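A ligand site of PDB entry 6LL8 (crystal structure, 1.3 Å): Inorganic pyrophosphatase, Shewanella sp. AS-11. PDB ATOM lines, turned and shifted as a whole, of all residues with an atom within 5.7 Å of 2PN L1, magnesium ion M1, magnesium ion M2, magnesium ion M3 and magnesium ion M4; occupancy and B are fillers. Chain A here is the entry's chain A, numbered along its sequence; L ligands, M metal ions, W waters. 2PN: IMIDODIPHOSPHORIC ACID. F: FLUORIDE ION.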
ATOM      1  N   HIS A   9     -23.472   7.230   5.003  1.00  0.00           N
ATOM      2  CA  HIS A   9     -24.436   7.709   5.993  1.00  0.00           C
ATOM      3  C   HIS A   9     -23.814   7.920   7.363  1.00  0.00           C
ATOM      4  O   HIS A   9     -22.848   7.255   7.746  1.00  0.00           O
ATOM      5  CB  HIS A   9     -25.698   6.834   6.061  1.00  0.00           C
ATOM      6  CG  HIS A   9     -25.522   5.356   6.219  1.00  0.00           C
ATOM      7  ND1 HIS A   9     -25.172   4.749   7.418  1.00  0.00           N
ATOM      8  CD2 HIS A   9     -25.727   4.344   5.336  1.00  0.00           C
ATOM      9  CE1 HIS A   9     -25.149   3.410   7.195  1.00  0.00           C
ATOM     10  NE2 HIS A   9     -25.480   3.138   5.929  1.00  0.00           N
ATOM     11  N   ASP A  13     -21.904   2.004   8.085  1.00  0.00           N
ATOM     12  CA  ASP A  13     -21.690   0.563   8.022  1.00  0.00           C
ATOM     13  C   ASP A  13     -20.613   0.242   6.985  1.00  0.00           C
ATOM     14  O   ASP A  13     -19.998   1.147   6.397  1.00  0.00           O
ATOM     15  CB  ASP A  13     -22.998  -0.136   7.773  1.00  0.00           C
ATOM     16  CG  ASP A  13     -23.735   0.360   6.536  1.00  0.00           C
ATOM     17  OD1 ASP A  13     -23.145   1.065   5.677  1.00  0.00           O
ATOM     18  OD2 ASP A  13     -24.946   0.042   6.378  1.00  0.00           O
ATOM     19  N   SER A  14     -20.377  -1.024   6.763  1.00  0.00           N
ATOM     20  CA  SER A  14     -19.308  -1.447   5.854  1.00  0.00           C
ATOM     21  C   SER A  14     -19.554  -0.903   4.448  1.00  0.00           C
ATOM     22  O   SER A  14     -18.574  -0.529   3.781  1.00  0.00           O
ATOM     23  CB  SER A  14     -19.119  -2.937   5.886  1.00  0.00           C
ATOM     24  OG  SER A  14     -18.739  -3.355   7.167  1.00  0.00           O
ATOM     25  N   ASP A  15     -20.762  -0.938   3.949  1.00  0.00           N
ATOM     26  CA  ASP A  15     -21.009  -0.406   2.606  1.00  0.00           C
ATOM     27  C   ASP A  15     -20.624   1.057   2.533  1.00  0.00           C
ATOM     28  O   ASP A  15     -19.957   1.486   1.575  1.00  0.00           O
ATOM     29  CB  ASP A  15     -22.478  -0.620   2.258  1.00  0.00           C
ATOM     30  CG  ASP A  15     -22.911  -0.434   0.832  1.00  0.00           C
ATOM     31  OD1 ASP A  15     -22.025  -0.553  -0.070  1.00  0.00           O
ATOM     32  OD2 ASP A  15     -24.120  -0.245   0.581  1.00  0.00           O
ATOM     33  N   SER A  16     -21.010   1.851   3.506  1.00  0.00           N
ATOM     34  CA  SER A  16     -20.691   3.280   3.528  1.00  0.00           C
ATOM     35  C   SER A  16     -19.183   3.514   3.623  1.00  0.00           C
ATOM     36  O   SER A  16     -18.695   4.477   3.038  1.00  0.00           O
ATOM     37  CB  SER A  16     -21.426   3.983   4.656  1.00  0.00           C
ATOM     38  OG  SER A  16     -22.758   4.332   4.321  1.00  0.00           O
ATOM     39  N   ASP A  73     -24.672   5.525  -0.337  1.00  0.00           N
ATOM     40  CA  ASP A  73     -25.439   4.573   0.499  1.00  0.00           C
ATOM     41  C   ASP A  73     -26.590   5.238   1.251  1.00  0.00           C
ATOM     42  O   ASP A  73     -27.083   4.622   2.207  1.00  0.00           O
ATOM     43  CB  ASP A  73     -24.508   3.794   1.409  1.00  0.00           C
ATOM     44  CG  ASP A  73     -25.037   2.600   2.130  1.00  0.00           C
ATOM     45  OD1 ASP A  73     -25.779   1.773   1.523  1.00  0.00           O
ATOM     46  OD2 ASP A  73     -24.643   2.453   3.301  1.00  0.00           O
ATOM     47  N   ASP A  94     -26.083   4.763  -4.695  1.00  0.00           N
ATOM     48  CA  ASP A  94     -26.946   4.232  -3.622  1.00  0.00           C
ATOM     49  C   ASP A  94     -27.842   3.140  -4.151  1.00  0.00           C
ATOM     50  O   ASP A  94     -27.920   2.877  -5.357  1.00  0.00           O
ATOM     51  CB  ASP A  94     -27.767   5.375  -3.004  1.00  0.00           C
ATOM     52  CG  ASP A  94     -28.493   5.020  -1.726  1.00  0.00           C
ATOM     53  OD1 ASP A  94     -28.025   4.065  -1.031  1.00  0.00           O
ATOM     54  OD2 ASP A  94     -29.488   5.675  -1.412  1.00  0.00           O
ATOM     55  N   HIS A  95     -28.588   2.550  -3.232  1.00  0.00           N
ATOM     56  CA  HIS A  95     -29.552   1.451  -3.469  1.00  0.00           C
ATOM     57  C   HIS A  95     -30.742   1.558  -2.510  1.00  0.00           C
ATOM     58  O   HIS A  95     -31.394   0.557  -2.237  1.00  0.00           O
ATOM     59  CB  HIS A  95     -28.846   0.102  -3.385  1.00  0.00           C
ATOM     60  CG  HIS A  95     -28.258  -0.269  -2.046  1.00  0.00           C
ATOM     61  ND1 HIS A  95     -28.373  -1.548  -1.563  1.00  0.00           N
ATOM     62  CD2 HIS A  95     -27.503   0.411  -1.139  1.00  0.00           C
ATOM     63  CE1 HIS A  95     -27.701  -1.602  -0.405  1.00  0.00           C
ATOM     64  NE2 HIS A  95     -27.160  -0.445  -0.108  1.00  0.00           N
ATOM     65  N   HIS A  96     -31.021   2.751  -2.007  1.00  0.00           N
ATOM     66  CA  HIS A  96     -32.181   3.041  -1.149  1.00  0.00           C
ATOM     67  C   HIS A  96     -33.276   3.764  -1.916  1.00  0.00           C
ATOM     68  O   HIS A  96     -33.056   4.230  -3.049  1.00  0.00           O
ATOM     69  CB  HIS A  96     -31.775   3.886   0.072  1.00  0.00           C
ATOM     70  CG  HIS A  96     -30.945   3.138   1.066  1.00  0.00           C
ATOM     71  ND1 HIS A  96     -29.560   3.002   0.957  1.00  0.00           N
ATOM     72  CD2 HIS A  96     -31.293   2.484   2.208  1.00  0.00           C
ATOM     73  CE1 HIS A  96     -29.135   2.271   1.980  1.00  0.00           C
ATOM     74  NE2 HIS A  96     -30.164   1.956   2.771  1.00  0.00           N
ATOM     75  N   GLY A 115     -28.567  -5.106  -4.119  1.00  0.00           N
ATOM     76  CA  GLY A 115     -28.240  -5.477  -2.738  1.00  0.00           C
ATOM     77  C   GLY A 115     -27.224  -4.632  -2.031  1.00  0.00           C
ATOM     78  O   GLY A 115     -27.205  -4.677  -0.816  1.00  0.00           O
ATOM     79  N   CYS A 116     -26.393  -3.877  -2.737  1.00  0.00           N
ATOM     80  CA  CYS A 116     -25.281  -3.171  -2.082  1.00  0.00           C
ATOM     81  C   CYS A 116     -24.843  -1.970  -2.911  1.00  0.00           C
ATOM     82  O   CYS A 116     -24.732  -2.103  -4.140  1.00  0.00           O
ATOM     83  CB  CYS A 116     -24.149  -4.146  -1.845  1.00  0.00           C
ATOM     84  SG  CYS A 116     -22.765  -3.451  -0.931  1.00  0.00           S
ATOM     85  N   SER A 117     -24.499  -0.856  -2.261  1.00  0.00           N
ATOM     86  CA  SER A 117     -23.955   0.272  -3.016  1.00  0.00           C
ATOM     87  C   SER A 117     -22.689  -0.130  -3.748  1.00  0.00           C
ATOM     88  O   SER A 117     -22.408   0.384  -4.845  1.00  0.00           O
ATOM     89  CB  SER A 117     -23.636   1.455  -2.115  1.00  0.00           C
ATOM     90  OG  SER A 117     -24.755   1.961  -1.440  1.00  0.00           O
ATOM     91  N   SER A 146     -22.004  -8.434   3.256  1.00  0.00           N
ATOM     92  CA  SER A 146     -22.648  -7.901   4.463  1.00  0.00           C
ATOM     93  C   SER A 146     -24.051  -7.401   4.121  1.00  0.00           C
ATOM     94  O   SER A 146     -25.034  -7.817   4.753  1.00  0.00           O
ATOM     95  CB  SER A 146     -21.807  -6.816   5.079  1.00  0.00           C
ATOM     96  OG  SER A 146     -22.376  -6.464   6.300  1.00  0.00           O
ATOM     97  N   ASP A 147     -24.150  -6.502   3.149  1.00  0.00           N
ATOM     98  CA  ASP A 147     -25.460  -5.915   2.816  1.00  0.00           C
ATOM     99  C   ASP A 147     -26.451  -6.959   2.337  1.00  0.00           C
ATOM    100  O   ASP A 147     -27.644  -6.834   2.625  1.00  0.00           O
ATOM    101  CB  ASP A 147     -25.302  -4.854   1.743  1.00  0.00           C
ATOM    102  CG  ASP A 147     -25.199  -3.454   2.291  1.00  0.00           C
ATOM    103  OD1 ASP A 147     -24.671  -3.323   3.389  1.00  0.00           O
ATOM    104  OD2 ASP A 147     -25.538  -2.476   1.575  1.00  0.00           O
ATOM    105  N   ASP A 202     -26.219   0.313  14.493  1.00  0.00           N
ATOM    106  CA  ASP A 202     -26.683   0.266  13.096  1.00  0.00           C
ATOM    107  C   ASP A 202     -28.038   0.954  13.051  1.00  0.00           C
ATOM    108  O   ASP A 202     -29.053   0.301  12.787  1.00  0.00           O
ATOM    109  CB  ASP A 202     -26.717  -1.155  12.603  1.00  0.00           C
ATOM    110  CG  ASP A 202     -27.126  -1.382  11.176  1.00  0.00           C
ATOM    111  OD1 ASP A 202     -27.225  -0.379  10.441  1.00  0.00           O
ATOM    112  OD2 ASP A 202     -27.254  -2.590  10.832  1.00  0.00           O
ATOM    113  N   LYS A 204     -30.576   4.334  12.141  1.00  0.00           N
ATOM    114  CA  LYS A 204     -30.879   5.398  11.187  1.00  0.00           C
ATOM    115  C   LYS A 204     -32.155   6.112  11.607  1.00  0.00           C
ATOM    116  O   LYS A 204     -33.120   5.468  12.007  1.00  0.00           O
ATOM    117  CB  LYS A 204     -31.090   4.836   9.783  1.00  0.00           C
ATOM    118  CG  LYS A 204     -29.827   4.216   9.196  1.00  0.00           C
ATOM    119  CD  LYS A 204     -30.115   3.585   7.841  1.00  0.00           C
ATOM    120  CE  LYS A 204     -28.861   2.965   7.232  1.00  0.00           C
ATOM    121  NZ  LYS A 204     -29.176   2.361   5.925  1.00  0.00           N
ATOM    122  N   PHE A 206     -35.267   8.477  10.170  1.00  0.00           N
ATOM    123  CA  PHE A 206     -36.099   8.699   8.980  1.00  0.00           C
ATOM    124  C   PHE A 206     -37.085   9.795   9.290  1.00  0.00           C
ATOM    125  O   PHE A 206     -37.761   9.762  10.328  1.00  0.00           O
ATOM    126  CB  PHE A 206     -36.864   7.436   8.619  1.00  0.00           C
ATOM    127  CG  PHE A 206     -35.972   6.292   8.246  1.00  0.00           C
ATOM    128  CD1 PHE A 206     -35.455   5.445   9.215  1.00  0.00           C
ATOM    129  CD2 PHE A 206     -35.569   6.100   6.934  1.00  0.00           C
ATOM    130  CE1 PHE A 206     -34.586   4.436   8.899  1.00  0.00           C
ATOM    131  CE2 PHE A 206     -34.721   5.063   6.604  1.00  0.00           C
ATOM    132  CZ  PHE A 206     -34.207   4.235   7.588  1.00  0.00           C
ATOM    133  N   GLN A 217     -30.871  -1.800  14.001  1.00  0.00           N
ATOM    134  CA  GLN A 217     -30.849  -3.220  13.626  1.00  0.00           C
ATOM    135  C   GLN A 217     -29.613  -3.872  14.208  1.00  0.00           C
ATOM    136  O   GLN A 217     -28.537  -3.269  14.196  1.00  0.00           O
ATOM    137  CB  GLN A 217     -30.898  -3.388  12.114  1.00  0.00           C
ATOM    138  CG  GLN A 217     -30.953  -4.861  11.692  1.00  0.00           C
ATOM    139  CD  GLN A 217     -31.291  -5.081  10.247  1.00  0.00           C
ATOM    140  OE1 GLN A 217     -30.924  -4.285   9.392  1.00  0.00           O
ATOM    141  NE2 GLN A 217     -32.026  -6.143   9.946  1.00  0.00           N
ATOM    142  N   GLU A 219     -28.041  -7.540  13.484  1.00  0.00           N
ATOM    143  CA  GLU A 219     -28.000  -8.828  12.786  1.00  0.00           C
ATOM    144  C   GLU A 219     -27.015  -9.748  13.483  1.00  0.00           C
ATOM    145  O   GLU A 219     -25.859  -9.382  13.723  1.00  0.00           O
ATOM    146  CB  GLU A 219     -27.513  -8.643  11.343  1.00  0.00           C
ATOM    147  CG  GLU A 219     -28.390  -7.798  10.437  1.00  0.00           C
ATOM    148  CD  GLU A 219     -27.568  -7.246   9.288  1.00  0.00           C
ATOM    149  OE1 GLU A 219     -26.540  -6.568   9.578  1.00  0.00           O
ATOM    150  OE2 GLU A 219     -27.880  -7.532   8.148  1.00  0.00           O
ATOM    151  N   SER A 293     -34.359  -7.298   5.785  1.00  0.00           N
ATOM    152  CA  SER A 293     -33.968  -6.033   5.151  1.00  0.00           C
ATOM    153  C   SER A 293     -34.754  -4.841   5.696  1.00  0.00           C
ATOM    154  O   SER A 293     -35.996  -4.786   5.529  1.00  0.00           O
ATOM    155  CB  SER A 293     -34.194  -6.124   3.690  1.00  0.00           C
ATOM    156  OG  SER A 293     -34.023  -4.854   3.072  1.00  0.00           O
ATOM    157  N   ARG A 294     -34.067  -3.865   6.253  1.00  0.00           N
ATOM    158  CA  ARG A 294     -34.731  -2.627   6.670  1.00  0.00           C
ATOM    159  C   ARG A 294     -35.226  -1.863   5.441  1.00  0.00           C
ATOM    160  O   ARG A 294     -36.403  -1.467   5.391  1.00  0.00           O
ATOM    161  CB  ARG A 294     -33.780  -1.832   7.569  1.00  0.00           C
ATOM    162  CG  ARG A 294     -34.308  -0.469   8.007  1.00  0.00           C
ATOM    163  CD  ARG A 294     -33.464   0.192   9.085  1.00  0.00           C
ATOM    164  NE  ARG A 294     -32.071   0.220   8.711  1.00  0.00           N
ATOM    165  CZ  ARG A 294     -31.036   0.193   9.535  1.00  0.00           C
ATOM    166  NH1 ARG A 294     -31.182   0.432  10.829  1.00  0.00           N
ATOM    167  NH2 ARG A 294     -29.833  -0.056   9.058  1.00  0.00           N
ATOM    168  N   LYS A 295     -34.383  -1.658   4.436  1.00  0.00           N
ATOM    169  CA  LYS A 295     -34.786  -0.827   3.284  1.00  0.00           C
ATOM    170  C   LYS A 295     -35.970  -1.450   2.519  1.00  0.00           C
ATOM    171  O   LYS A 295     -36.756  -0.700   1.960  1.00  0.00           O
ATOM    172  CB  LYS A 295     -33.640  -0.542   2.308  1.00  0.00           C
ATOM    173  CG  LYS A 295     -33.187  -1.728   1.485  1.00  0.00           C
ATOM    174  CD  LYS A 295     -32.161  -1.383   0.388  1.00  0.00           C
ATOM    175  CE  LYS A 295     -30.869  -0.796   0.891  1.00  0.00           C
ATOM    176  NZ  LYS A 295     -30.145  -1.710   1.814  1.00  0.00           N
ATOM    177  N   LYS A 296     -36.076  -2.785   2.472  1.00  0.00           N
ATOM    178  CA  LYS A 296     -37.071  -3.408   1.589  1.00  0.00           C
ATOM    179  C   LYS A 296     -38.286  -3.890   2.357  1.00  0.00           C
ATOM    180  O   LYS A 296     -39.401  -3.851   1.818  1.00  0.00           O
ATOM    181  CB  LYS A 296     -36.436  -4.543   0.785  1.00  0.00           C
ATOM    182  CG  LYS A 296     -37.287  -5.163  -0.280  1.00  0.00           C
ATOM    183  CD  LYS A 296     -36.518  -6.140  -1.127  1.00  0.00           C
ATOM    184  CE  LYS A 296     -37.368  -6.920  -2.110  1.00  0.00           C
ATOM    185  NZ  LYS A 296     -38.005  -6.047  -3.093  1.00  0.00           N
HETATM  186  P1  2PN L   1     -27.881  -0.425   4.208  1.00  0.00           P
HETATM  187  O1  2PN L   1     -27.254   0.899   4.661  1.00  0.00           O
HETATM  188  O2  2PN L   1     -27.413  -1.590   5.044  1.00  0.00           O
HETATM  189  O3  2PN L   1     -27.654  -0.647   2.727  1.00  0.00           O
HETATM  190  N1  2PN L   1     -29.502  -0.267   4.425  1.00  0.00           N
HETATM  191  P2  2PN L   1     -30.614  -0.930   5.445  1.00  0.00           P
HETATM  192  O4  2PN L   1     -31.351   0.275   6.022  1.00  0.00           O
HETATM  193  O5  2PN L   1     -29.868  -1.680   6.528  1.00  0.00           O
HETATM  194  O6  2PN L   1     -31.526  -1.817   4.635  1.00  0.00           O
HETATM  195  F     F L   2     -25.058  -0.304   3.565  1.00  0.00           F
HETATM  196 MG    MG M   1     -25.324   1.265   4.752  1.00  0.00          MG
HETATM  197 MG    MG M   2     -25.884  -0.367   1.738  1.00  0.00          MG
HETATM  198 MG    MG M   3     -27.991  -2.466   6.733  1.00  0.00          MG
HETATM  199 MG    MG M   4     -25.175  -1.972   5.042  1.00  0.00          MG
HETATM  200  O   HOH W   1     -28.590  -4.286   5.804  1.00  0.00           O
HETATM  201  O   HOH W   2     -27.144  -0.855   7.779  1.00  0.00           O
HETATM  202  O   HOH W   3     -28.451  -3.265   8.586  1.00  0.00           O
HETATM  203  O   HOH W   4     -26.030  -3.374   6.766  1.00  0.00           O
HETATM  204  O   HOH W   5     -22.869  -2.643   5.257  1.00  0.00           O
HETATM  205  O   HOH W   6     -33.241   1.953   5.164  1.00  0.00           O
HETATM  206  O   HOH W   7     -31.466  -4.209   3.365  1.00  0.00           O
HETATM  207  O   HOH W   8     -28.141  -3.726   3.100  1.00  0.00           O
HETATM  208  O   HOH W   9     -31.293  -4.157   6.722  1.00  0.00           O
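NZ of Lys 204 is in salt-bridge range of O4 of 2PN L1 (3.0 Å).
NE of Arg 294 is in salt-bridge range of O4 of 2PN L1 (2.8 Å).
A nitrogen (N1) of 2PN L1 sits at hydrogen-bond distance from a ring nitrogen (NE2) of His 96, 2.8 Å away.
The backbone NH (N) of Lys 295 is in hydrogen-bond range of an oxygen (O6) of 2PN L1.
O6 of 2PN L1 lies within salt-bridge range of NZ of Lys 295, at 3.1 Å.
A ring nitrogen (ND1) of His 96 sits close to the backbone carbonyl oxygen (O) of Asp 73 (3.2 Å).
OD2 of Asp 73 sits close to OG of Ser 16.
The side-chain carboxylate (OD1) of Asp 73 sits close to the side-chain hydroxyl (OG) of Ser 117.
The backbone NH (N) of Ser 117 lies close to the side-chain carboxylate (OD1) of Asp 15, at 3.3 Å.
SG of Cys 116 is in hydrogen-bond range of OD1 of Asp 15 (3.1 Å).
The backbone carbonyl oxygen (O) of Gly 115 lies close to a ring nitrogen (ND1) of His 95 (3.4 Å).
NE2 of His 96 is in hydrogen-bond range of NZ of Lys 204, 3.3 Å away.
N of Lys 295 lies close to OG of Ser 293 (3.5 Å).
Of the 23 residues printed, 9 come within 4 Å of 2PN L1.
Within 4 Å of magnesium ion M1: His 9, Asp 13 and Asp 73.
Within 4 Å of magnesium ion M2: Asp 15, Asp 73, His 95 and Asp 147.
Merely in contact with magnesium ion M3: Arg 294 (3.8 Å).
Of the 23 residues printed, 2 come within 4 Å of magnesium ion M3.
O1 of 2PN L1 binds magnesium ion M1 (2.0 Å).
Magnesium ion M1 is bound by F of F L2 (2.0 Å).
OD2 of Asp 73 binds magnesium ion M1, at 2.0 Å.
Magnesium ion M1 is bound by OD2 of Asp 13.
NE2 of His 9 is bound to magnesium ion M1, at 2.2 Å.
OD1 of Asp 13 is bound to magnesium ion M1, 2.4 Å away.
Magnesium ion M1 has six donor atoms within binding distance.
Magnesium ion M2 is bound by F of F L2, O3 of 2PN L1, OD2 of Asp 15, OD2 of Asp 147, OD1 of Asp 73 and NE2 of His 95.
Magnesium ion M3 is bound by O2 of 2PN L1 (2.0 Å), O5 of 2PN L1 (2.0 Å), water W3 (2.1 Å), water W2 (2.1 Å), water W1 (2.1 Å) and water W4 (2.2 Å).
Magnesium ion M4 is bound by OD1 of Asp 147, F of F L2, O2 of 2PN L1, water W4, water W5 and OD2 of Asp 13.
Water W2 lies within hydrogen-bond range of the side-chain carboxylate (OD1) of Asp 202 (2.7 Å) and the guanidinium group (NH2) of Arg 294 (3.1 Å).
Water W3 lies within hydrogen-bond range of OD2 of Asp 202 (2.6 Å) and OE1 of Gln 217 (2.8 Å).
Water W7 lies within hydrogen-bond range of OG of Ser 293, O6 of 2PN L1 and NZ of Lys 295.
Water W9 lies within hydrogen-bond range of OE1 of Gln 217 (2.7 Å), N of Arg 294 (2.8 Å) and O6 of 2PN L1 (3.1 Å).
Water W8 bridges NZ of Lys 295 (3.1 Å) and O of Asp 147 (3.2 Å).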
